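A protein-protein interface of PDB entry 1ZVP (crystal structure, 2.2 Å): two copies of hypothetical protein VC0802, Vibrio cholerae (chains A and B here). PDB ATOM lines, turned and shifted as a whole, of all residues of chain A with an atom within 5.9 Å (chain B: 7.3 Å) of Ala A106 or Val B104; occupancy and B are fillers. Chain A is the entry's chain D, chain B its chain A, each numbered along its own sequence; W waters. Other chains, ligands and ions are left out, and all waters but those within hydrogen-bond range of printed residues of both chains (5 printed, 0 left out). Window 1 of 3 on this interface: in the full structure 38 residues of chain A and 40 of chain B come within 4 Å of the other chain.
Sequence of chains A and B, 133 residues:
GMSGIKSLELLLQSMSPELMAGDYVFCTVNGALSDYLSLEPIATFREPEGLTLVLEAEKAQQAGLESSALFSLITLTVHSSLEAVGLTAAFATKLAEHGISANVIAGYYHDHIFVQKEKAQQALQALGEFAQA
The backbone carbonyl oxygen of Asn B103 is in hydrogen-bond range of the backbone NH of Phe B114 (2.9 Å).
N of Ile A105 lies within hydrogen-bond range of O of His A112 (2.7 Å).
The backbone carbonyl oxygen of His A110 lies within hydrogen-bond range of a ring nitrogen (NE2) of His A112 (3.2 Å).
The backbone carbonyl oxygen of Phe B45 lies within hydrogen-bond range of the backbone NH of Thr B52 (2.7 Å).
The side-chain hydroxyl (OG1) of Thr B52 lies within hydrogen-bond range of the side-chain carboxylate (OE1) of Glu B47, at 3.3 Å.
The backbone NH of Ile B105 lies within hydrogen-bond range of the backbone carbonyl oxygen of His B112, at 2.8 Å.
Thr A88 touches Val B104, but with the chains exchanged Val A104 does not touch Thr B88 (4.4 Å).
Val B104 touches its own counterpart, Val A104.
Val A104 touches Ile B105, and with the chains exchanged Ile A105 touches Val B104.
Ile B105 touches its own counterpart, Ile A105.
Positions printed for both chains: 88, 91, 104, 105, 106, 107, 111 and 112.
Of the 22 pairs that touch across the chains among the printed residues, 6 have their exchanged pair printed and touching as well.
Printed residues of chain B that touch a printed residue of chain A: Phe B26, Phe B45, Glu B47, Thr B52, Ala B92, Ser B101, Ala B102, Asn B103, Val B104, Ile B105 and Ala B106.
Hydrophobic or aromatic side chains of chain B that line the printed part of chain A: Phe B26, Phe B45, Ala B92, Val B104, Ile B105 and Ala B106.
Printed residues of chain A that touch a printed residue of chain B: Leu A82, Thr A88, Val A104, Ile A105, Ala A106, Gly A107, Tyr A108, His A110 and His A112.
Hydrophobic or aromatic side chains of chain A within 4 Å of the printed part of chain B: Leu A82, Val A104, Ile A105, Ala A106, Tyr A108 and His A112.
Among the printed residues, no Asp or Glu carboxylate lies within 4 Å of a Lys or Arg side-chain nitrogen of the other chain.
Of the printed residues of chain B, Ile A105 touches Phe B45, Val B104 and Ile B105.
Ala A106 touches just these residues of chain B: Phe B26, Asn B103 and Val B104.
Of the printed residues of chain B, Gly A107 touches Glu B47 (3.4 Å) and Thr B52 (3.8 Å).
Of chain A, only Thr A88 (3.7 Å), Val A104 (3.2 Å), Ile A105 (3.4 Å) and Ala A106 (2.7 Å) come within 4 Å of Val B104.
Ile B113 touches none of the printed residues of chain A.
The nearest residue of chain B that does not touch Ala A106 is Ile B105 (4.05 Å).
The nearest residue of chain A that does not touch Val B104 is Asp A111 (5.3 Å).
The nearest printed residue of chain A that does not touch Glu B47 is Asp A111 (5.3 Å).
Thr A88 touches Ala B92.
CG1 of Val B104 touches CG2 of Thr A88, 3.7 Å away.
CA of Ile B105 touches O of Val A104 (3.4 Å).
Ile A105 touches Val B104.
Phe B26 touches Ala A106.
Ala A106 touches Asn B103 (CB to CB, 3.97 Å).
CA of Gly A107 touches OE2 of Glu B47, 3.4 Å away.
Thr B52 touches Gly A107.
Tyr A108 touches Phe B26.
His A112 touches Phe B45.
Water W2 lies within hydrogen-bond range of OD1 of Asn B103 (2.6 Å) and OD1 of Asp A111 (2.9 Å).
Water W3 bridges the side-chain carboxylate (OD1) of Asp B111 (2.7 Å) and the backbone NH (N) of Val A104 (3.0 Å).
Water W1 lies within hydrogen-bond range of OD1 of Asp A111 (2.9 Å), N of Val B104 (3.0 Å), OG1 of Thr A88 (3.1 Å) and O of Ala B102 (3.2 Å).
Water W5 lies within hydrogen-bond range of ND1 of His A110 (3.0 Å) and OE2 of Glu B47 (3.4 Å).
Water W4 lies within hydrogen-bond range of N of Ala B102 (3.4 Å) and OG1 of Thr A88 (3.5 Å).
N of Ala B106 sits at hydrogen-bond distance from O of Val A104, at 2.7 Å.
N of Ala A106 sits at hydrogen-bond distance from O of Val B104 (2.7 Å).
The backbone NH of Tyr A108 sits at hydrogen-bond distance from the side-chain hydroxyl of Thr B52, 2.9 Å away.
ND2 of Asn B103 sits at hydrogen-bond distance from O of Leu A82.
The side-chain carboxylate (OE1) of Glu B47 sits at hydrogen-bond distance from the backbone NH (N) of Tyr A108 (3.4 Å).
The side-chain carboxylate of Glu B47 is in hydrogen-bond range of the backbone NH of His A110.
The backbone carbonyl oxygen (O) of Leu A82 is in hydrogen-bond range of the side-chain hydroxyl (OG) of Ser B101, at 3.4 Å.
OG1 of Thr A88 sits at hydrogen-bond distance from O of Ala B102 (2.6 Å).
The backbone carbonyl oxygen of Val A104 sits close to the backbone carbonyl oxygen of Val B104 (3.2 Å).
The side-chain carboxylate (OE2) of Glu B47 is in hydrogen-bond range of a ring nitrogen (NE2) of His A112 (2.7 Å).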
ATOM      1  N   LEU A  82     -25.763  21.303  13.773  1.00  0.00           N
ATOM      2  CA  LEU A  82     -25.569  20.065  12.989  1.00  0.00           C
ATOM      3  C   LEU A  82     -24.079  19.735  12.708  1.00  0.00           C
ATOM      4  O   LEU A  82     -23.760  18.789  11.971  1.00  0.00           O
ATOM      5  CB  LEU A  82     -26.388  20.102  11.674  1.00  0.00           C
ATOM      6  CG  LEU A  82     -27.900  19.819  11.568  1.00  0.00           C
ATOM      7  CD1 LEU A  82     -28.383  18.664  12.451  1.00  0.00           C
ATOM      8  CD2 LEU A  82     -28.693  21.060  11.856  1.00  0.00           C
ATOM      9  N   THR A  88     -23.333  13.755  20.105  1.00  0.00           N
ATOM     10  CA  THR A  88     -23.983  12.451  19.976  1.00  0.00           C
ATOM     11  C   THR A  88     -23.311  11.427  20.871  1.00  0.00           C
ATOM     12  O   THR A  88     -23.990  10.644  21.535  1.00  0.00           O
ATOM     13  CB  THR A  88     -24.030  11.963  18.524  1.00  0.00           C
ATOM     14  OG1 THR A  88     -24.679  12.960  17.722  1.00  0.00           O
ATOM     15  CG2 THR A  88     -24.816  10.671  18.430  1.00  0.00           C
ATOM     16  N   PHE A  91     -24.461  12.241  24.742  1.00  0.00           N
ATOM     17  CA  PHE A  91     -25.778  11.742  25.143  1.00  0.00           C
ATOM     18  C   PHE A  91     -25.960  10.234  25.006  1.00  0.00           C
ATOM     19  O   PHE A  91     -26.554   9.607  25.889  1.00  0.00           O
ATOM     20  CB  PHE A  91     -26.965  12.565  24.589  1.00  0.00           C
ATOM     21  CG  PHE A  91     -27.237  12.410  23.121  1.00  0.00           C
ATOM     22  CD1 PHE A  91     -26.973  13.453  22.247  1.00  0.00           C
ATOM     23  CD2 PHE A  91     -27.833  11.262  22.614  1.00  0.00           C
ATOM     24  CE1 PHE A  91     -27.257  13.335  20.883  1.00  0.00           C
ATOM     25  CE2 PHE A  91     -28.110  11.136  21.264  1.00  0.00           C
ATOM     26  CZ  PHE A  91     -27.831  12.177  20.398  1.00  0.00           C
ATOM     27  N   VAL A 104     -32.099   7.580  18.020  1.00  0.00           N
ATOM     28  CA  VAL A 104     -31.856   9.000  17.885  1.00  0.00           C
ATOM     29  C   VAL A 104     -32.394   9.479  16.547  1.00  0.00           C
ATOM     30  O   VAL A 104     -32.123   8.855  15.522  1.00  0.00           O
ATOM     31  CB  VAL A 104     -30.332   9.249  17.907  1.00  0.00           C
ATOM     32  CG1 VAL A 104     -29.993  10.710  17.649  1.00  0.00           C
ATOM     33  CG2 VAL A 104     -29.714   8.722  19.196  1.00  0.00           C
ATOM     34  N   ILE A 105     -33.172  10.566  16.544  1.00  0.00           N
ATOM     35  CA  ILE A 105     -33.400  11.303  15.300  1.00  0.00           C
ATOM     36  C   ILE A 105     -32.922  12.740  15.450  1.00  0.00           C
ATOM     37  O   ILE A 105     -33.444  13.490  16.271  1.00  0.00           O
ATOM     38  CB  ILE A 105     -34.864  11.235  14.782  1.00  0.00           C
ATOM     39  CG1 ILE A 105     -35.352   9.779  14.749  1.00  0.00           C
ATOM     40  CG2 ILE A 105     -34.968  11.896  13.397  1.00  0.00           C
ATOM     41  CD1 ILE A 105     -36.727   9.575  14.162  1.00  0.00           C
ATOM     42  N   ALA A 106     -31.900  13.105  14.680  1.00  0.00           N
ATOM     43  CA  ALA A 106     -31.401  14.481  14.651  1.00  0.00           C
ATOM     44  C   ALA A 106     -32.373  15.354  13.866  1.00  0.00           C
ATOM     45  O   ALA A 106     -32.642  15.095  12.684  1.00  0.00           O
ATOM     46  CB  ALA A 106     -30.002  14.553  14.039  1.00  0.00           C
ATOM     47  N   GLY A 107     -32.927  16.363  14.534  1.00  0.00           N
ATOM     48  CA  GLY A 107     -33.771  17.352  13.871  1.00  0.00           C
ATOM     49  C   GLY A 107     -32.890  18.527  13.505  1.00  0.00           C
ATOM     50  O   GLY A 107     -31.710  18.559  13.871  1.00  0.00           O
ATOM     51  N   TYR A 108     -33.448  19.490  12.778  1.00  0.00           N
ATOM     52  CA  TYR A 108     -32.702  20.694  12.423  1.00  0.00           C
ATOM     53  C   TYR A 108     -32.215  21.459  13.660  1.00  0.00           C
ATOM     54  O   TYR A 108     -31.048  21.882  13.711  1.00  0.00           O
ATOM     55  CB  TYR A 108     -33.553  21.605  11.552  1.00  0.00           C
ATOM     56  CG  TYR A 108     -32.800  22.793  11.029  1.00  0.00           C
ATOM     57  CD1 TYR A 108     -32.193  22.744   9.782  1.00  0.00           C
ATOM     58  CD2 TYR A 108     -32.684  23.963  11.779  1.00  0.00           C
ATOM     59  CE1 TYR A 108     -31.488  23.824   9.283  1.00  0.00           C
ATOM     60  CE2 TYR A 108     -31.978  25.061  11.294  1.00  0.00           C
ATOM     61  CZ  TYR A 108     -31.384  24.980  10.037  1.00  0.00           C
ATOM     62  OH  TYR A 108     -30.681  26.041   9.510  1.00  0.00           O
ATOM     63  N   HIS A 110     -32.902  20.360  17.295  1.00  0.00           N
ATOM     64  CA  HIS A 110     -32.477  19.543  18.424  1.00  0.00           C
ATOM     65  C   HIS A 110     -32.410  18.069  18.086  1.00  0.00           C
ATOM     66  O   HIS A 110     -33.026  17.619  17.135  1.00  0.00           O
ATOM     67  CB  HIS A 110     -33.433  19.715  19.606  1.00  0.00           C
ATOM     68  CG  HIS A 110     -33.519  21.113  20.134  1.00  0.00           C
ATOM     69  ND1 HIS A 110     -34.560  21.964  19.825  1.00  0.00           N
ATOM     70  CD2 HIS A 110     -32.695  21.808  20.957  1.00  0.00           C
ATOM     71  CE1 HIS A 110     -34.375  23.119  20.434  1.00  0.00           C
ATOM     72  NE2 HIS A 110     -33.251  23.050  21.129  1.00  0.00           N
ATOM     73  N   ASP A 111     -31.671  17.321  18.893  1.00  0.00           N
ATOM     74  CA  ASP A 111     -31.726  15.870  18.846  1.00  0.00           C
ATOM     75  C   ASP A 111     -32.938  15.367  19.604  1.00  0.00           C
ATOM     76  O   ASP A 111     -33.282  15.881  20.670  1.00  0.00           O
ATOM     77  CB  ASP A 111     -30.463  15.258  19.437  1.00  0.00           C
ATOM     78  CG  ASP A 111     -29.256  15.495  18.577  1.00  0.00           C
ATOM     79  OD1 ASP A 111     -29.227  14.980  17.434  1.00  0.00           O
ATOM     80  OD2 ASP A 111     -28.326  16.194  19.041  1.00  0.00           O
ATOM     81  N   HIS A 112     -33.573  14.353  19.041  1.00  0.00           N
ATOM     82  CA  HIS A 112     -34.738  13.728  19.640  1.00  0.00           C
ATOM     83  C   HIS A 112     -34.430  12.254  19.840  1.00  0.00           C
ATOM     84  O   HIS A 112     -33.929  11.582  18.940  1.00  0.00           O
ATOM     85  CB  HIS A 112     -35.961  13.920  18.741  1.00  0.00           C
ATOM     86  CG  HIS A 112     -36.144  15.333  18.275  1.00  0.00           C
ATOM     87  ND1 HIS A 112     -36.792  16.288  19.030  1.00  0.00           N
ATOM     88  CD2 HIS A 112     -35.742  15.957  17.143  1.00  0.00           C
ATOM     89  CE1 HIS A 112     -36.789  17.438  18.378  1.00  0.00           C
ATOM     90  NE2 HIS A 112     -36.158  17.265  17.232  1.00  0.00           N
ATOM     91  N   PHE B  26     -29.856  19.614   5.674  1.00  0.00           N
ATOM     92  CA  PHE B  26     -30.949  19.780   6.630  1.00  0.00           C
ATOM     93  C   PHE B  26     -31.590  21.132   6.409  1.00  0.00           C
ATOM     94  O   PHE B  26     -30.902  22.155   6.365  1.00  0.00           O
ATOM     95  CB  PHE B  26     -30.434  19.682   8.064  1.00  0.00           C
ATOM     96  CG  PHE B  26     -30.194  18.277   8.529  1.00  0.00           C
ATOM     97  CD1 PHE B  26     -31.012  17.707   9.494  1.00  0.00           C
ATOM     98  CD2 PHE B  26     -29.154  17.520   8.004  1.00  0.00           C
ATOM     99  CE1 PHE B  26     -30.802  16.406   9.931  1.00  0.00           C
ATOM    100  CE2 PHE B  26     -28.937  16.210   8.429  1.00  0.00           C
ATOM    101  CZ  PHE B  26     -29.762  15.652   9.396  1.00  0.00           C
ATOM    102  N   ALA B  43     -35.750  12.079   4.666  1.00  0.00           N
ATOM    103  CA  ALA B  43     -36.096  12.086   6.079  1.00  0.00           C
ATOM    104  C   ALA B  43     -36.915  13.308   6.453  1.00  0.00           C
ATOM    105  O   ALA B  43     -36.822  14.357   5.833  1.00  0.00           O
ATOM    106  CB  ALA B  43     -34.842  12.000   6.950  1.00  0.00           C
ATOM    107  N   THR B  44     -37.690  13.150   7.513  1.00  0.00           N
ATOM    108  CA  THR B  44     -38.682  14.113   7.954  1.00  0.00           C
ATOM    109  C   THR B  44     -38.738  14.052   9.488  1.00  0.00           C
ATOM    110  O   THR B  44     -38.693  12.966  10.068  1.00  0.00           O
ATOM    111  CB  THR B  44     -40.041  13.745   7.291  1.00  0.00           C
ATOM    112  OG1 THR B  44     -40.173  14.463   6.063  1.00  0.00           O
ATOM    113  CG2 THR B  44     -41.209  14.045   8.152  1.00  0.00           C
ATOM    114  N   PHE B  45     -38.776  15.205  10.149  1.00  0.00           N
ATOM    115  CA  PHE B  45     -39.100  15.248  11.574  1.00  0.00           C
ATOM    116  C   PHE B  45     -39.913  16.496  11.875  1.00  0.00           C
ATOM    117  O   PHE B  45     -39.533  17.603  11.507  1.00  0.00           O
ATOM    118  CB  PHE B  45     -37.855  15.154  12.490  1.00  0.00           C
ATOM    119  CG  PHE B  45     -38.195  14.820  13.924  1.00  0.00           C
ATOM    120  CD1 PHE B  45     -38.102  13.516  14.390  1.00  0.00           C
ATOM    121  CD2 PHE B  45     -38.665  15.797  14.793  1.00  0.00           C
ATOM    122  CE1 PHE B  45     -38.444  13.188  15.700  1.00  0.00           C
ATOM    123  CE2 PHE B  45     -39.020  15.477  16.107  1.00  0.00           C
ATOM    124  CZ  PHE B  45     -38.907  14.165  16.557  1.00  0.00           C
ATOM    125  N   GLU B  47     -40.634  19.031  14.337  1.00  0.00           N
ATOM    126  CA  GLU B  47     -40.198  19.688  15.570  1.00  0.00           C
ATOM    127  C   GLU B  47     -41.243  20.754  15.946  1.00  0.00           C
ATOM    128  O   GLU B  47     -41.960  21.242  15.077  1.00  0.00           O
ATOM    129  CB  GLU B  47     -38.825  20.342  15.379  1.00  0.00           C
ATOM    130  CG  GLU B  47     -37.690  19.393  15.004  1.00  0.00           C
ATOM    131  CD  GLU B  47     -36.297  20.047  15.105  1.00  0.00           C
ATOM    132  OE1 GLU B  47     -36.046  21.042  14.387  1.00  0.00           O
ATOM    133  OE2 GLU B  47     -35.452  19.566  15.902  1.00  0.00           O
ATOM    134  N   THR B  52     -38.593  19.527   9.943  1.00  0.00           N
ATOM    135  CA  THR B  52     -37.259  19.223   9.430  1.00  0.00           C
ATOM    136  C   THR B  52     -37.383  18.405   8.157  1.00  0.00           C
ATOM    137  O   THR B  52     -38.051  17.364   8.138  1.00  0.00           O
ATOM    138  CB  THR B  52     -36.381  18.449  10.442  1.00  0.00           C
ATOM    139  OG1 THR B  52     -36.065  19.292  11.550  1.00  0.00           O
ATOM    140  CG2 THR B  52     -35.078  17.984   9.794  1.00  0.00           C
ATOM    141  N   VAL B  54     -34.815  16.508   5.442  1.00  0.00           N
ATOM    142  CA  VAL B  54     -33.484  16.112   4.989  1.00  0.00           C
ATOM    143  C   VAL B  54     -33.609  15.727   3.517  1.00  0.00           C
ATOM    144  O   VAL B  54     -34.269  14.749   3.170  1.00  0.00           O
ATOM    145  CB  VAL B  54     -32.865  14.956   5.831  1.00  0.00           C
ATOM    146  CG1 VAL B  54     -31.462  14.642   5.354  1.00  0.00           C
ATOM    147  CG2 VAL B  54     -32.831  15.323   7.296  1.00  0.00           C
ATOM    148  N   THR B  88     -24.536   3.019  19.683  1.00  0.00           N
ATOM    149  CA  THR B  88     -24.529   4.440  19.306  1.00  0.00           C
ATOM    150  C   THR B  88     -23.378   5.186  19.970  1.00  0.00           C
ATOM    151  O   THR B  88     -22.713   5.999  19.325  1.00  0.00           O
ATOM    152  CB  THR B  88     -25.860   5.170  19.639  1.00  0.00           C
ATOM    153  OG1 THR B  88     -26.975   4.369  19.252  1.00  0.00           O
ATOM    154  CG2 THR B  88     -25.943   6.510  18.926  1.00  0.00           C
ATOM    155  N   PHE B  91     -19.977   4.121  17.965  1.00  0.00           N
ATOM    156  CA  PHE B  91     -19.692   4.704  16.662  1.00  0.00           C
ATOM    157  C   PHE B  91     -19.594   6.225  16.690  1.00  0.00           C
ATOM    158  O   PHE B  91     -18.808   6.797  15.937  1.00  0.00           O
ATOM    159  CB  PHE B  91     -20.587   4.167  15.528  1.00  0.00           C
ATOM    160  CG  PHE B  91     -21.997   4.694  15.520  1.00  0.00           C
ATOM    161  CD1 PHE B  91     -22.269   6.019  15.186  1.00  0.00           C
ATOM    162  CD2 PHE B  91     -23.065   3.838  15.763  1.00  0.00           C
ATOM    163  CE1 PHE B  91     -23.584   6.502  15.157  1.00  0.00           C
ATOM    164  CE2 PHE B  91     -24.382   4.301  15.725  1.00  0.00           C
ATOM    165  CZ  PHE B  91     -24.645   5.639  15.421  1.00  0.00           C
ATOM    166  N   ALA B  92     -20.361   6.862  17.578  1.00  0.00           N
ATOM    167  CA  ALA B  92     -20.327   8.316  17.748  1.00  0.00           C
ATOM    168  C   ALA B  92     -19.033   8.770  18.416  1.00  0.00           C
ATOM    169  O   ALA B  92     -18.488   9.814  18.051  1.00  0.00           O
ATOM    170  CB  ALA B  92     -21.534   8.802  18.518  1.00  0.00           C
ATOM    171  N   LEU B  95     -16.236   8.524  15.787  1.00  0.00           N
ATOM    172  CA  LEU B  95     -16.321   9.684  14.913  1.00  0.00           C
ATOM    173  C   LEU B  95     -15.876  10.963  15.616  1.00  0.00           C
ATOM    174  O   LEU B  95     -15.191  11.786  15.010  1.00  0.00           O
ATOM    175  CB  LEU B  95     -17.727   9.843  14.349  1.00  0.00           C
ATOM    176  CG  LEU B  95     -18.246   8.774  13.386  1.00  0.00           C
ATOM    177  CD1 LEU B  95     -19.729   8.964  13.194  1.00  0.00           C
ATOM    178  CD2 LEU B  95     -17.505   8.798  12.063  1.00  0.00           C
ATOM    179  N   SER B 101     -18.664  15.134  13.448  1.00  0.00           N
ATOM    180  CA  SER B 101     -19.953  15.160  14.124  1.00  0.00           C
ATOM    181  C   SER B 101     -20.908  14.177  13.455  1.00  0.00           C
ATOM    182  O   SER B 101     -20.903  14.034  12.242  1.00  0.00           O
ATOM    183  CB  SER B 101     -20.532  16.575  14.159  1.00  0.00           C
ATOM    184  OG  SER B 101     -20.996  16.972  12.880  1.00  0.00           O
ATOM    185  N   ALA B 102     -21.701  13.482  14.259  1.00  0.00           N
ATOM    186  CA  ALA B 102     -22.611  12.459  13.767  1.00  0.00           C
ATOM    187  C   ALA B 102     -24.016  12.966  13.981  1.00  0.00           C
ATOM    188  O   ALA B 102     -24.415  13.227  15.111  1.00  0.00           O
ATOM    189  CB  ALA B 102     -22.402  11.148  14.528  1.00  0.00           C
ATOM    190  N   ASN B 103     -24.762  13.138  12.904  1.00  0.00           N
ATOM    191  CA  ASN B 103     -26.163  13.450  13.029  1.00  0.00           C
ATOM    192  C   ASN B 103     -26.951  12.222  12.685  1.00  0.00           C
ATOM    193  O   ASN B 103     -27.138  11.928  11.512  1.00  0.00           O
ATOM    194  CB  ASN B 103     -26.526  14.608  12.113  1.00  0.00           C
ATOM    195  CG  ASN B 103     -25.731  15.847  12.433  1.00  0.00           C
ATOM    196  OD1 ASN B 103     -25.934  16.479  13.473  1.00  0.00           O
ATOM    197  ND2 ASN B 103     -24.803  16.194  11.553  1.00  0.00           N
ATOM    198  N   VAL B 104     -27.401  11.491  13.701  1.00  0.00           N
ATOM    199  CA  VAL B 104     -28.068  10.212  13.450  1.00  0.00           C
ATOM    200  C   VAL B 104     -29.591  10.277  13.317  1.00  0.00           C
ATOM    201  O   VAL B 104     -30.277  11.002  14.039  1.00  0.00           O
ATOM    202  CB  VAL B 104     -27.494   9.028  14.336  1.00  0.00           C
ATOM    203  CG1 VAL B 104     -26.463   9.529  15.334  1.00  0.00           C
ATOM    204  CG2 VAL B 104     -28.574   8.154  14.962  1.00  0.00           C
ATOM    205  N   ILE B 105     -30.095   9.577  12.309  1.00  0.00           N
ATOM    206  CA  ILE B 105     -31.530   9.350  12.170  1.00  0.00           C
ATOM    207  C   ILE B 105     -31.750   7.848  12.187  1.00  0.00           C
ATOM    208  O   ILE B 105     -31.302   7.150  11.289  1.00  0.00           O
ATOM    209  CB  ILE B 105     -32.127   9.995  10.885  1.00  0.00           C
ATOM    210  CG1 ILE B 105     -31.925  11.523  10.923  1.00  0.00           C
ATOM    211  CG2 ILE B 105     -33.608   9.626  10.744  1.00  0.00           C
ATOM    212  CD1 ILE B 105     -32.444  12.305   9.718  1.00  0.00           C
ATOM    213  N   ALA B 106     -32.390   7.353  13.242  1.00  0.00           N
ATOM    214  CA  ALA B 106     -32.765   5.949  13.329  1.00  0.00           C
ATOM    215  C   ALA B 106     -33.915   5.650  12.362  1.00  0.00           C
ATOM    216  O   ALA B 106     -34.991   6.258  12.444  1.00  0.00           O
ATOM    217  CB  ALA B 106     -33.151   5.594  14.757  1.00  0.00           C
ATOM    218  N   GLY B 107     -33.672   4.745  11.414  1.00  0.00           N
ATOM    219  CA  GLY B 107     -34.739   4.214  10.571  1.00  0.00           C
ATOM    220  C   GLY B 107     -35.241   2.928  11.200  1.00  0.00           C
ATOM    221  O   GLY B 107     -34.739   2.512  12.250  1.00  0.00           O
ATOM    222  N   ASP B 111     -29.563   2.411  11.480  1.00  0.00           N
ATOM    223  CA  ASP B 111     -29.090   3.731  11.869  1.00  0.00           C
ATOM    224  C   ASP B 111     -28.502   4.429  10.644  1.00  0.00           C
ATOM    225  O   ASP B 111     -27.744   3.834   9.884  1.00  0.00           O
ATOM    226  CB  ASP B 111     -27.993   3.597  12.929  1.00  0.00           C
ATOM    227  CG  ASP B 111     -28.519   3.706  14.356  1.00  0.00           C
ATOM    228  OD1 ASP B 111     -29.590   4.312  14.573  1.00  0.00           O
ATOM    229  OD2 ASP B 111     -27.832   3.196  15.271  1.00  0.00           O
ATOM    230  N   HIS B 112     -28.841   5.690  10.452  1.00  0.00           N
ATOM    231  CA  HIS B 112     -28.318   6.443   9.332  1.00  0.00           C
ATOM    232  C   HIS B 112     -27.578   7.640   9.884  1.00  0.00           C
ATOM    233  O   HIS B 112     -28.138   8.406  10.660  1.00  0.00           O
ATOM    234  CB  HIS B 112     -29.464   6.868   8.419  1.00  0.00           C
ATOM    235  CG  HIS B 112     -30.240   5.714   7.877  1.00  0.00           C
ATOM    236  ND1 HIS B 112     -31.437   5.301   8.421  1.00  0.00           N
ATOM    237  CD2 HIS B 112     -29.967   4.851   6.870  1.00  0.00           C
ATOM    238  CE1 HIS B 112     -31.881   4.251   7.759  1.00  0.00           C
ATOM    239  NE2 HIS B 112     -31.007   3.956   6.813  1.00  0.00           N
ATOM    240  N   ILE B 113     -26.313   7.785   9.508  1.00  0.00           N
ATOM    241  CA  ILE B 113     -25.467   8.854  10.038  1.00  0.00           C
ATOM    242  C   ILE B 113     -25.185   9.905   8.974  1.00  0.00           C
ATOM    243  O   ILE B 113     -24.708   9.590   7.889  1.00  0.00           O
ATOM    244  CB  ILE B 113     -24.117   8.315  10.593  1.00  0.00           C
ATOM    245  CG1 ILE B 113     -24.346   7.114  11.521  1.00  0.00           C
ATOM    246  CG2 ILE B 113     -23.356   9.419  11.315  1.00  0.00           C
ATOM    247  CD1 ILE B 113     -23.122   6.193  11.655  1.00  0.00           C
ATOM    248  N   PHE B 114     -25.478  11.159   9.290  1.00  0.00           N
ATOM    249  CA  PHE B 114     -25.115  12.262   8.413  1.00  0.00           C
ATOM    250  C   PHE B 114     -23.849  12.954   8.918  1.00  0.00           C
ATOM    251  O   PHE B 114     -23.804  13.491  10.029  1.00  0.00           O
ATOM    252  CB  PHE B 114     -26.300  13.222   8.243  1.00  0.00           C
ATOM    253  CG  PHE B 114     -27.471  12.599   7.521  1.00  0.00           C
ATOM    254  CD1 PHE B 114     -27.645  12.796   6.155  1.00  0.00           C
ATOM    255  CD2 PHE B 114     -28.380  11.786   8.206  1.00  0.00           C
ATOM    256  CE1 PHE B 114     -28.715  12.207   5.487  1.00  0.00           C
ATOM    257  CE2 PHE B 114     -29.438  11.192   7.561  1.00  0.00           C
ATOM    258  CZ  PHE B 114     -29.616  11.401   6.198  1.00  0.00           C
HETATM  259  O   HOH W   1     -27.400  13.014  16.266  1.00  0.00           O
HETATM  260  O   HOH W   2     -27.633  16.442  15.453  1.00  0.00           O
HETATM  261  O   HOH W   3     -30.263   5.595  16.825  1.00  0.00           O
HETATM  262  O   HOH W   4     -22.238  15.332  17.094  1.00  0.00           O
HETATM  263  O   HOH W   5     -37.053  20.692  18.701  1.00  0.00           O
